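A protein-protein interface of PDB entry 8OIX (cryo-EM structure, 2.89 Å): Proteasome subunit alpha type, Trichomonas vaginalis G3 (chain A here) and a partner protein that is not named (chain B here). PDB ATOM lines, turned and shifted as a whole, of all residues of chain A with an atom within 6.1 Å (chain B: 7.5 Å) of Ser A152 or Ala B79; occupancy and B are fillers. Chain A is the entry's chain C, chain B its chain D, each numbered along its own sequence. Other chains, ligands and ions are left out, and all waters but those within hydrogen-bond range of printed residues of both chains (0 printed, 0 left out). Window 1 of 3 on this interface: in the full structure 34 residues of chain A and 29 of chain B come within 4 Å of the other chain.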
ATOM      1  N   ILE A  18       3.784 -30.271  10.090  1.00  0.00           N
ATOM      2  CA  ILE A  18       4.242 -31.435  10.842  1.00  0.00           C
ATOM      3  C   ILE A  18       4.082 -32.656   9.945  1.00  0.00           C
ATOM      4  O   ILE A  18       2.961 -33.043   9.608  1.00  0.00           O
ATOM      5  CB  ILE A  18       3.463 -31.611  12.152  1.00  0.00           C
ATOM      6  CG1 ILE A  18       3.586 -30.377  13.045  1.00  0.00           C
ATOM      7  CG2 ILE A  18       3.944 -32.842  12.883  1.00  0.00           C
ATOM      8  CD1 ILE A  18       2.464 -29.384  12.869  1.00  0.00           C
ATOM      9  N   VAL A  21       1.679 -35.238  10.995  1.00  0.00           N
ATOM     10  CA  VAL A  21       0.275 -34.917  10.790  1.00  0.00           C
ATOM     11  C   VAL A  21      -0.095 -35.084   9.326  1.00  0.00           C
ATOM     12  O   VAL A  21      -1.210 -35.507   9.007  1.00  0.00           O
ATOM     13  CB  VAL A  21      -0.017 -33.490  11.276  1.00  0.00           C
ATOM     14  CG1 VAL A  21      -1.452 -33.117  10.982  1.00  0.00           C
ATOM     15  CG2 VAL A  21       0.284 -33.371  12.749  1.00  0.00           C
ATOM     16  N   ILE A  25      -2.849 -37.654   7.960  1.00  0.00           N
ATOM     17  CA  ILE A  25      -3.889 -37.269   7.011  1.00  0.00           C
ATOM     18  C   ILE A  25      -3.891 -38.210   5.813  1.00  0.00           C
ATOM     19  O   ILE A  25      -4.953 -38.606   5.318  1.00  0.00           O
ATOM     20  CB  ILE A  25      -3.705 -35.800   6.588  1.00  0.00           C
ATOM     21  CG1 ILE A  25      -4.038 -34.867   7.753  1.00  0.00           C
ATOM     22  CG2 ILE A  25      -4.566 -35.474   5.382  1.00  0.00           C
ATOM     23  CD1 ILE A  25      -3.614 -33.433   7.532  1.00  0.00           C
ATOM     24  N   CYS A 114      -9.945 -32.077  19.627  1.00  0.00           N
ATOM     25  CA  CYS A 114      -8.934 -31.461  18.786  1.00  0.00           C
ATOM     26  C   CYS A 114      -7.788 -30.909  19.617  1.00  0.00           C
ATOM     27  O   CYS A 114      -6.653 -30.879  19.142  1.00  0.00           O
ATOM     28  CB  CYS A 114      -9.560 -30.362  17.931  1.00  0.00           C
ATOM     29  SG  CYS A 114     -10.690 -30.987  16.681  1.00  0.00           S
ATOM     30  N   ASP A 115      -8.049 -30.511  20.864  1.00  0.00           N
ATOM     31  CA  ASP A 115      -6.960 -30.158  21.764  1.00  0.00           C
ATOM     32  C   ASP A 115      -6.121 -31.379  22.102  1.00  0.00           C
ATOM     33  O   ASP A 115      -4.893 -31.292  22.159  1.00  0.00           O
ATOM     34  CB  ASP A 115      -7.506 -29.517  23.038  1.00  0.00           C
ATOM     35  CG  ASP A 115      -8.000 -28.104  22.817  1.00  0.00           C
ATOM     36  OD1 ASP A 115      -7.548 -27.458  21.848  1.00  0.00           O
ATOM     37  OD2 ASP A 115      -8.838 -27.637  23.615  1.00  0.00           O
ATOM     38  N   LYS A 117      -5.754 -34.046  20.139  1.00  0.00           N
ATOM     39  CA  LYS A 117      -5.020 -34.389  18.927  1.00  0.00           C
ATOM     40  C   LYS A 117      -3.902 -33.397  18.654  1.00  0.00           C
ATOM     41  O   LYS A 117      -2.834 -33.790  18.179  1.00  0.00           O
ATOM     42  CB  LYS A 117      -5.973 -34.451  17.735  1.00  0.00           C
ATOM     43  CG  LYS A 117      -6.956 -35.603  17.792  1.00  0.00           C
ATOM     44  CD  LYS A 117      -7.407 -36.033  16.405  1.00  0.00           C
ATOM     45  CE  LYS A 117      -8.779 -35.480  16.067  1.00  0.00           C
ATOM     46  NZ  LYS A 117      -8.795 -33.995  16.057  1.00  0.00           N
ATOM     47  N   HIS A 118      -4.116 -32.118  18.968  1.00  0.00           N
ATOM     48  CA  HIS A 118      -3.085 -31.112  18.760  1.00  0.00           C
ATOM     49  C   HIS A 118      -1.951 -31.275  19.761  1.00  0.00           C
ATOM     50  O   HIS A 118      -0.778 -31.130  19.404  1.00  0.00           O
ATOM     51  CB  HIS A 118      -3.694 -29.718  18.864  1.00  0.00           C
ATOM     52  CG  HIS A 118      -2.696 -28.651  19.174  1.00  0.00           C
ATOM     53  ND1 HIS A 118      -1.854 -28.125  18.219  1.00  0.00           N
ATOM     54  CD2 HIS A 118      -2.401 -28.014  20.331  1.00  0.00           C
ATOM     55  CE1 HIS A 118      -1.082 -27.209  18.776  1.00  0.00           C
ATOM     56  NE2 HIS A 118      -1.394 -27.122  20.056  1.00  0.00           N
ATOM     57  N   SER A 119      -2.287 -31.539  21.026  1.00  0.00           N
ATOM     58  CA  SER A 119      -1.267 -31.787  22.035  1.00  0.00           C
ATOM     59  C   SER A 119      -0.371 -32.935  21.609  1.00  0.00           C
ATOM     60  O   SER A 119       0.840 -32.916  21.859  1.00  0.00           O
ATOM     61  CB  SER A 119      -1.922 -32.083  23.383  1.00  0.00           C
ATOM     62  OG  SER A 119      -2.774 -33.210  23.297  1.00  0.00           O
ATOM     63  N   THR A 121       0.421 -33.401  18.623  1.00  0.00           N
ATOM     64  CA  THR A 121       1.223 -32.852  17.536  1.00  0.00           C
ATOM     65  C   THR A 121       2.189 -31.763  17.981  1.00  0.00           C
ATOM     66  O   THR A 121       3.014 -31.326  17.174  1.00  0.00           O
ATOM     67  CB  THR A 121       0.325 -32.291  16.426  1.00  0.00           C
ATOM     68  OG1 THR A 121      -0.260 -31.055  16.856  1.00  0.00           O
ATOM     69  CG2 THR A 121      -0.759 -33.274  16.074  1.00  0.00           C
ATOM     70  N   GLN A 122       2.108 -31.313  19.231  1.00  0.00           N
ATOM     71  CA  GLN A 122       2.960 -30.231  19.707  1.00  0.00           C
ATOM     72  C   GLN A 122       3.792 -30.582  20.929  1.00  0.00           C
ATOM     73  O   GLN A 122       4.819 -29.930  21.155  1.00  0.00           O
ATOM     74  CB  GLN A 122       2.117 -28.989  20.036  1.00  0.00           C
ATOM     75  CG  GLN A 122       2.932 -27.716  20.207  1.00  0.00           C
ATOM     76  CD  GLN A 122       2.080 -26.469  20.262  1.00  0.00           C
ATOM     77  OE1 GLN A 122       0.950 -26.498  20.743  1.00  0.00           O
ATOM     78  NE2 GLN A 122       2.616 -25.365  19.760  1.00  0.00           N
ATOM     79  N   TYR A 129      -2.743 -38.653  16.604  1.00  0.00           N
ATOM     80  CA  TYR A 129      -3.947 -39.458  16.427  1.00  0.00           C
ATOM     81  C   TYR A 129      -4.325 -39.433  14.953  1.00  0.00           C
ATOM     82  O   TYR A 129      -4.869 -38.445  14.454  1.00  0.00           O
ATOM     83  CB  TYR A 129      -5.082 -38.933  17.295  1.00  0.00           C
ATOM     84  CG  TYR A 129      -4.985 -39.324  18.750  1.00  0.00           C
ATOM     85  CD1 TYR A 129      -5.246 -40.625  19.155  1.00  0.00           C
ATOM     86  CD2 TYR A 129      -4.650 -38.391  19.719  1.00  0.00           C
ATOM     87  CE1 TYR A 129      -5.168 -40.988  20.482  1.00  0.00           C
ATOM     88  CE2 TYR A 129      -4.571 -38.746  21.050  1.00  0.00           C
ATOM     89  CZ  TYR A 129      -4.828 -40.046  21.426  1.00  0.00           C
ATOM     90  OH  TYR A 129      -4.749 -40.406  22.751  1.00  0.00           O
ATOM     91  N   ASP A 150      -9.200 -32.967  12.383  1.00  0.00           N
ATOM     92  CA  ASP A 150      -7.993 -33.425  11.716  1.00  0.00           C
ATOM     93  C   ASP A 150      -7.004 -33.932  12.753  1.00  0.00           C
ATOM     94  O   ASP A 150      -7.125 -33.615  13.942  1.00  0.00           O
ATOM     95  CB  ASP A 150      -7.355 -32.292  10.896  1.00  0.00           C
ATOM     96  CG  ASP A 150      -8.291 -31.737   9.841  1.00  0.00           C
ATOM     97  OD1 ASP A 150      -9.108 -32.511   9.300  1.00  0.00           O
ATOM     98  OD2 ASP A 150      -8.208 -30.526   9.553  1.00  0.00           O
ATOM     99  N   PRO A 151      -6.020 -34.738  12.341  1.00  0.00           N
ATOM    100  CA  PRO A 151      -4.951 -35.113  13.280  1.00  0.00           C
ATOM    101  C   PRO A 151      -4.183 -33.923  13.815  1.00  0.00           C
ATOM    102  O   PRO A 151      -3.638 -33.995  14.923  1.00  0.00           O
ATOM    103  CB  PRO A 151      -4.049 -36.026  12.440  1.00  0.00           C
ATOM    104  CG  PRO A 151      -4.921 -36.540  11.380  1.00  0.00           C
ATOM    105  CD  PRO A 151      -5.887 -35.442  11.055  1.00  0.00           C
ATOM    106  N   SER A 152      -4.119 -32.828  13.054  1.00  0.00           N
ATOM    107  CA  SER A 152      -3.474 -31.614  13.537  1.00  0.00           C
ATOM    108  C   SER A 152      -4.196 -31.017  14.729  1.00  0.00           C
ATOM    109  O   SER A 152      -3.603 -30.222  15.465  1.00  0.00           O
ATOM    110  CB  SER A 152      -3.397 -30.576  12.417  1.00  0.00           C
ATOM    111  OG  SER A 152      -4.691 -30.153  12.025  1.00  0.00           O
ATOM    112  N   GLY A 153      -5.451 -31.390  14.946  1.00  0.00           N
ATOM    113  CA  GLY A 153      -6.272 -30.724  15.929  1.00  0.00           C
ATOM    114  C   GLY A 153      -7.076 -29.576  15.378  1.00  0.00           C
ATOM    115  O   GLY A 153      -7.535 -28.732  16.152  1.00  0.00           O
ATOM    116  N   ASN A 154      -7.252 -29.508  14.062  1.00  0.00           N
ATOM    117  CA  ASN A 154      -8.040 -28.463  13.428  1.00  0.00           C
ATOM    118  C   ASN A 154      -9.422 -29.015  13.125  1.00  0.00           C
ATOM    119  O   ASN A 154      -9.551 -30.124  12.598  1.00  0.00           O
ATOM    120  CB  ASN A 154      -7.376 -27.977  12.139  1.00  0.00           C
ATOM    121  CG  ASN A 154      -6.037 -27.319  12.384  1.00  0.00           C
ATOM    122  OD1 ASN A 154      -5.761 -26.841  13.481  1.00  0.00           O
ATOM    123  ND2 ASN A 154      -5.196 -27.291  11.358  1.00  0.00           N
ATOM    124  N   PHE B  60     -16.598 -20.574  11.827  1.00  0.00           N
ATOM    125  CA  PHE B  60     -15.297 -20.837  12.437  1.00  0.00           C
ATOM    126  C   PHE B  60     -14.405 -19.639  12.136  1.00  0.00           C
ATOM    127  O   PHE B  60     -13.902 -19.487  11.020  1.00  0.00           O
ATOM    128  CB  PHE B  60     -14.695 -22.132  11.905  1.00  0.00           C
ATOM    129  CG  PHE B  60     -13.400 -22.512  12.562  1.00  0.00           C
ATOM    130  CD1 PHE B  60     -13.394 -23.206  13.761  1.00  0.00           C
ATOM    131  CD2 PHE B  60     -12.187 -22.173  11.985  1.00  0.00           C
ATOM    132  CE1 PHE B  60     -12.206 -23.558  14.370  1.00  0.00           C
ATOM    133  CE2 PHE B  60     -10.994 -22.520  12.591  1.00  0.00           C
ATOM    134  CZ  PHE B  60     -11.005 -23.213  13.784  1.00  0.00           C
ATOM    135  N   PHE B  74      -5.430 -14.567  14.445  1.00  0.00           N
ATOM    136  CA  PHE B  74      -4.249 -15.392  14.265  1.00  0.00           C
ATOM    137  C   PHE B  74      -4.078 -15.758  12.802  1.00  0.00           C
ATOM    138  O   PHE B  74      -5.030 -15.754  12.019  1.00  0.00           O
ATOM    139  CB  PHE B  74      -4.311 -16.671  15.109  1.00  0.00           C
ATOM    140  CG  PHE B  74      -5.427 -17.607  14.724  1.00  0.00           C
ATOM    141  CD1 PHE B  74      -5.291 -18.480  13.653  1.00  0.00           C
ATOM    142  CD2 PHE B  74      -6.590 -17.652  15.469  1.00  0.00           C
ATOM    143  CE1 PHE B  74      -6.306 -19.349  13.316  1.00  0.00           C
ATOM    144  CE2 PHE B  74      -7.609 -18.523  15.135  1.00  0.00           C
ATOM    145  CZ  PHE B  74      -7.467 -19.370  14.058  1.00  0.00           C
ATOM    146  N   GLY B  76      -1.916 -19.036  10.867  1.00  0.00           N
ATOM    147  CA  GLY B  76      -1.095 -20.214  11.054  1.00  0.00           C
ATOM    148  C   GLY B  76      -1.916 -21.452  11.336  1.00  0.00           C
ATOM    149  O   GLY B  76      -3.066 -21.555  10.901  1.00  0.00           O
ATOM    150  N   LEU B  77      -1.330 -22.403  12.058  1.00  0.00           N
ATOM    151  CA  LEU B  77      -2.034 -23.625  12.417  1.00  0.00           C
ATOM    152  C   LEU B  77      -3.223 -23.296  13.308  1.00  0.00           C
ATOM    153  O   LEU B  77      -3.069 -22.660  14.353  1.00  0.00           O
ATOM    154  CB  LEU B  77      -1.081 -24.586  13.123  1.00  0.00           C
ATOM    155  CG  LEU B  77       0.171 -24.979  12.336  1.00  0.00           C
ATOM    156  CD1 LEU B  77       0.876 -26.138  13.008  1.00  0.00           C
ATOM    157  CD2 LEU B  77      -0.177 -25.325  10.897  1.00  0.00           C
ATOM    158  N   HIS B  78      -4.413 -23.742  12.906  1.00  0.00           N
ATOM    159  CA  HIS B  78      -5.606 -23.441  13.687  1.00  0.00           C
ATOM    160  C   HIS B  78      -5.597 -24.109  15.056  1.00  0.00           C
ATOM    161  O   HIS B  78      -6.223 -23.591  15.983  1.00  0.00           O
ATOM    162  CB  HIS B  78      -6.857 -23.853  12.912  1.00  0.00           C
ATOM    163  CG  HIS B  78      -6.932 -23.267  11.537  1.00  0.00           C
ATOM    164  ND1 HIS B  78      -7.677 -23.834  10.526  1.00  0.00           N
ATOM    165  CD2 HIS B  78      -6.353 -22.165  11.005  1.00  0.00           C
ATOM    166  CE1 HIS B  78      -7.554 -23.107   9.431  1.00  0.00           C
ATOM    167  NE2 HIS B  78      -6.755 -22.088   9.694  1.00  0.00           N
ATOM    168  N   ALA B  79      -4.883 -25.226  15.215  1.00  0.00           N
ATOM    169  CA  ALA B  79      -4.835 -25.884  16.516  1.00  0.00           C
ATOM    170  C   ALA B  79      -3.837 -25.210  17.449  1.00  0.00           C
ATOM    171  O   ALA B  79      -4.121 -25.029  18.640  1.00  0.00           O
ATOM    172  CB  ALA B  79      -4.490 -27.359  16.342  1.00  0.00           C
ATOM    173  N   ASP B  80      -2.675 -24.813  16.927  1.00  0.00           N
ATOM    174  CA  ASP B  80      -1.733 -24.064  17.749  1.00  0.00           C
ATOM    175  C   ASP B  80      -2.319 -22.715  18.117  1.00  0.00           C
ATOM    176  O   ASP B  80      -2.122 -22.226  19.236  1.00  0.00           O
ATOM    177  CB  ASP B  80      -0.409 -23.879  17.009  1.00  0.00           C
ATOM    178  CG  ASP B  80       0.290 -25.188  16.725  1.00  0.00           C
ATOM    179  OD1 ASP B  80      -0.307 -26.044  16.041  1.00  0.00           O
ATOM    180  OD2 ASP B  80       1.439 -25.362  17.183  1.00  0.00           O
ATOM    181  N   ALA B  81      -3.094 -22.136  17.205  1.00  0.00           N
ATOM    182  CA  ALA B  81      -3.788 -20.893  17.498  1.00  0.00           C
ATOM    183  C   ALA B  81      -4.884 -21.107  18.526  1.00  0.00           C
ATOM    184  O   ALA B  81      -5.097 -20.256  19.388  1.00  0.00           O
ATOM    185  CB  ALA B  81      -4.369 -20.313  16.220  1.00  0.00           C
ATOM    186  N   ARG B  82      -5.604 -22.225  18.444  1.00  0.00           N
ATOM    187  CA  ARG B  82      -6.620 -22.496  19.451  1.00  0.00           C
ATOM    188  C   ARG B  82      -5.989 -22.638  20.826  1.00  0.00           C
ATOM    189  O   ARG B  82      -6.537 -22.151  21.820  1.00  0.00           O
ATOM    190  CB  ARG B  82      -7.412 -23.750  19.097  1.00  0.00           C
ATOM    191  CG  ARG B  82      -8.679 -23.899  19.916  1.00  0.00           C
ATOM    192  CD  ARG B  82      -9.353 -25.228  19.668  1.00  0.00           C
ATOM    193  NE  ARG B  82      -9.348 -25.578  18.254  1.00  0.00           N
ATOM    194  CZ  ARG B  82      -8.610 -26.541  17.725  1.00  0.00           C
ATOM    195  NH1 ARG B  82      -7.816 -27.293  18.469  1.00  0.00           N
ATOM    196  NH2 ARG B  82      -8.670 -26.759  16.415  1.00  0.00           N
ATOM    197  N   ARG B  83      -4.837 -23.305  20.904  1.00  0.00           N
ATOM    198  CA  ARG B  83      -4.145 -23.414  22.184  1.00  0.00           C
ATOM    199  C   ARG B  83      -3.691 -22.046  22.681  1.00  0.00           C
ATOM    200  O   ARG B  83      -3.828 -21.733  23.871  1.00  0.00           O
ATOM    201  CB  ARG B  83      -2.958 -24.369  22.069  1.00  0.00           C
ATOM    202  CG  ARG B  83      -2.535 -24.951  23.406  1.00  0.00           C
ATOM    203  CD  ARG B  83      -1.293 -25.811  23.291  1.00  0.00           C
ATOM    204  NE  ARG B  83      -0.952 -26.430  24.566  1.00  0.00           N
ATOM    205  CZ  ARG B  83      -1.478 -27.562  25.015  1.00  0.00           C
ATOM    206  NH1 ARG B  83      -2.378 -28.231  24.314  1.00  0.00           N
ATOM    207  NH2 ARG B  83      -1.090 -28.034  26.196  1.00  0.00           N
ATOM    208  N   LEU B  84      -3.156 -21.212  21.783  1.00  0.00           N
ATOM    209  CA  LEU B  84      -2.751 -19.864  22.173  1.00  0.00           C
ATOM    210  C   LEU B  84      -3.938 -19.053  22.678  1.00  0.00           C
ATOM    211  O   LEU B  84      -3.830 -18.349  23.685  1.00  0.00           O
ATOM    212  CB  LEU B  84      -2.085 -19.146  21.000  1.00  0.00           C
ATOM    213  CG  LEU B  84      -0.611 -19.439  20.737  1.00  0.00           C
ATOM    214  CD1 LEU B  84      -0.101 -18.581  19.595  1.00  0.00           C
ATOM    215  CD2 LEU B  84       0.208 -19.203  21.992  1.00  0.00           C
ATOM    216  N   ILE B  85      -5.076 -19.138  21.990  1.00  0.00           N
ATOM    217  CA  ILE B  85      -6.252 -18.363  22.374  1.00  0.00           C
ATOM    218  C   ILE B  85      -6.820 -18.869  23.693  1.00  0.00           C
ATOM    219  O   ILE B  85      -7.245 -18.080  24.544  1.00  0.00           O
ATOM    220  CB  ILE B  85      -7.302 -18.390  21.244  1.00  0.00           C
ATOM    221  CG1 ILE B  85      -7.075 -17.244  20.252  1.00  0.00           C
ATOM    222  CG2 ILE B  85      -8.712 -18.329  21.803  1.00  0.00           C
ATOM    223  CD1 ILE B  85      -5.854 -17.374  19.382  1.00  0.00           C
ATOM    224  N   ARG B 126       6.826 -28.112  20.446  1.00  0.00           N
ATOM    225  CA  ARG B 126       6.930 -27.600  19.087  1.00  0.00           C
ATOM    226  C   ARG B 126       6.520 -26.136  19.056  1.00  0.00           C
ATOM    227  O   ARG B 126       5.429 -25.805  19.539  1.00  0.00           O
ATOM    228  CB  ARG B 126       6.044 -28.388  18.142  1.00  0.00           C
ATOM    229  CG  ARG B 126       6.288 -28.059  16.680  1.00  0.00           C
ATOM    230  CD  ARG B 126       5.357 -28.823  15.753  1.00  0.00           C
ATOM    231  NE  ARG B 126       3.981 -28.911  16.234  1.00  0.00           N
ATOM    232  CZ  ARG B 126       3.167 -27.878  16.411  1.00  0.00           C
ATOM    233  NH1 ARG B 126       3.542 -26.643  16.127  1.00  0.00           N
ATOM    234  NH2 ARG B 126       1.935 -28.094  16.862  1.00  0.00           N
ATOM    235  N   TYR B 128       4.835 -22.711  18.412  1.00  0.00           N
ATOM    236  CA  TYR B 128       3.529 -22.428  17.839  1.00  0.00           C
ATOM    237  C   TYR B 128       3.693 -21.940  16.409  1.00  0.00           C
ATOM    238  O   TYR B 128       4.365 -20.935  16.160  1.00  0.00           O
ATOM    239  CB  TYR B 128       2.792 -21.384  18.673  1.00  0.00           C
ATOM    240  CG  TYR B 128       2.256 -21.903  19.985  1.00  0.00           C
ATOM    241  CD1 TYR B 128       0.992 -22.466  20.066  1.00  0.00           C
ATOM    242  CD2 TYR B 128       3.004 -21.804  21.147  1.00  0.00           C
ATOM    243  CE1 TYR B 128       0.495 -22.933  21.265  1.00  0.00           C
ATOM    244  CE2 TYR B 128       2.515 -22.264  22.350  1.00  0.00           C
ATOM    245  CZ  TYR B 128       1.261 -22.829  22.404  1.00  0.00           C
ATOM    246  OH  TYR B 128       0.774 -23.289  23.605  1.00  0.00           O
ATOM    247  N   VAL B 130       2.011 -20.198  14.715  1.00  0.00           N
ATOM    248  CA  VAL B 130       0.973 -19.177  14.676  1.00  0.00           C
ATOM    249  C   VAL B 130       1.597 -17.827  14.990  1.00  0.00           C
ATOM    250  O   VAL B 130       2.368 -17.698  15.946  1.00  0.00           O
ATOM    251  CB  VAL B 130      -0.158 -19.484  15.676  1.00  0.00           C
ATOM    252  CG1 VAL B 130      -1.084 -18.290  15.828  1.00  0.00           C
ATOM    253  CG2 VAL B 130      -0.919 -20.696  15.231  1.00  0.00           C
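The side-chain carboxylate of Asp A115 lies within salt-bridge range of the guanidinium group of Arg B82 (3.4 Å). A ring nitrogen (ND1) of His A118 sits close to the side-chain carboxylate (OD1) of Asp B80, at 3.4 Å. The guanidinium group (NE) of Arg B126 sits at hydrogen-bond distance from the backbone carbonyl oxygen (O) of Thr A121 (2.8 Å). The side-chain carboxylate (OD2) of Asp B80 is in hydrogen-bond range of the side-chain amide nitrogen (NE2) of Gln A122 (2.8 Å). The backbone carbonyl oxygen (O) of Gln A122 sits at hydrogen-bond distance from the backbone NH (N) of Arg B126 (2.8 Å). The backbone carbonyl oxygen (O) of Gly A153 is in hydrogen-bond range of the guanidinium group (NH1) of Arg B82. N of His B78 sits close to OD1 of Asn A154, 3.4 Å away. The backbone NH (N) of Ala B79 lies within hydrogen-bond range of the side-chain amide oxygen (OD1) of Asn A154, at 2.5 Å.
The side-chain sulfur (SG) of Cys A114 lies within hydrogen-bond range of the side-chain amino group (NZ) of Lys A117, at 3.6 Å. The side-chain hydroxyl (OG) of Ser A119 is in hydrogen-bond range of the backbone carbonyl oxygen (O) of Asp A115 (3.1 Å). O of His A118 sits at hydrogen-bond distance from OG1 of Thr A121, 2.6 Å away. NE2 of His A118 lies within hydrogen-bond range of OE1 of Gln A122 (2.5 Å). OG of Ser A152 lies within hydrogen-bond range of ND2 of Asn A154 (3.0 Å). OD2 of Asp B80 lies within salt-bridge range of NH1 of Arg B126 (2.7 Å).
Arg B126 touches Ile A18. Arg B82 touches Cys A114 (NH1 to CB, 3.6 Å). ND1 of His A118 touches CB of Ala B79, 3.3 Å away. Arg B83 touches His A118 (CD to NE2, 3.5 Å). Ser A119 touches Arg B83. Arg B83 touches Gln A122 (CD to OE1, 3.5 Å). Tyr B128 touches Gln A122 (CD1 to NE2, 3.3 Å). Ser A152 touches Ala B79 (O to CB, 3.1 Å). CB of Ala B79 touches O of Gly A153, at 3.3 Å. Asn A154 touches Arg B82 (CA to NH2, 3.5 Å).
Ser A152 touches just one residue of chain B: Ala B79 (3.1 Å). Of chain B, only Ala B79 and Arg B82 come within 4 Å of Gly A153. Printed residues of chain A within 4 Å of Leu B77: Ile A18 (3.6 Å). Of the printed residues of chain A, His B78 touches Asn A154. Of chain A, only His A118 (3.3 Å), Ser A152 (3.1 Å), Gly A153 (3.3 Å) and Asn A154 (2.5 Å) come within 4 Å of Ala B79. The nearest residue of chain B that does not touch Ser A152 is Asp B80 (5.4 Å).
Of the 16 printed residues of chain A, 10 touch a printed residue of chain B. Printed residues of chain B that touch a printed residue of chain A: Leu B77, His B78, Ala B79, Asp B80, Arg B82, Arg B83, Arg B126 and Tyr B128.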
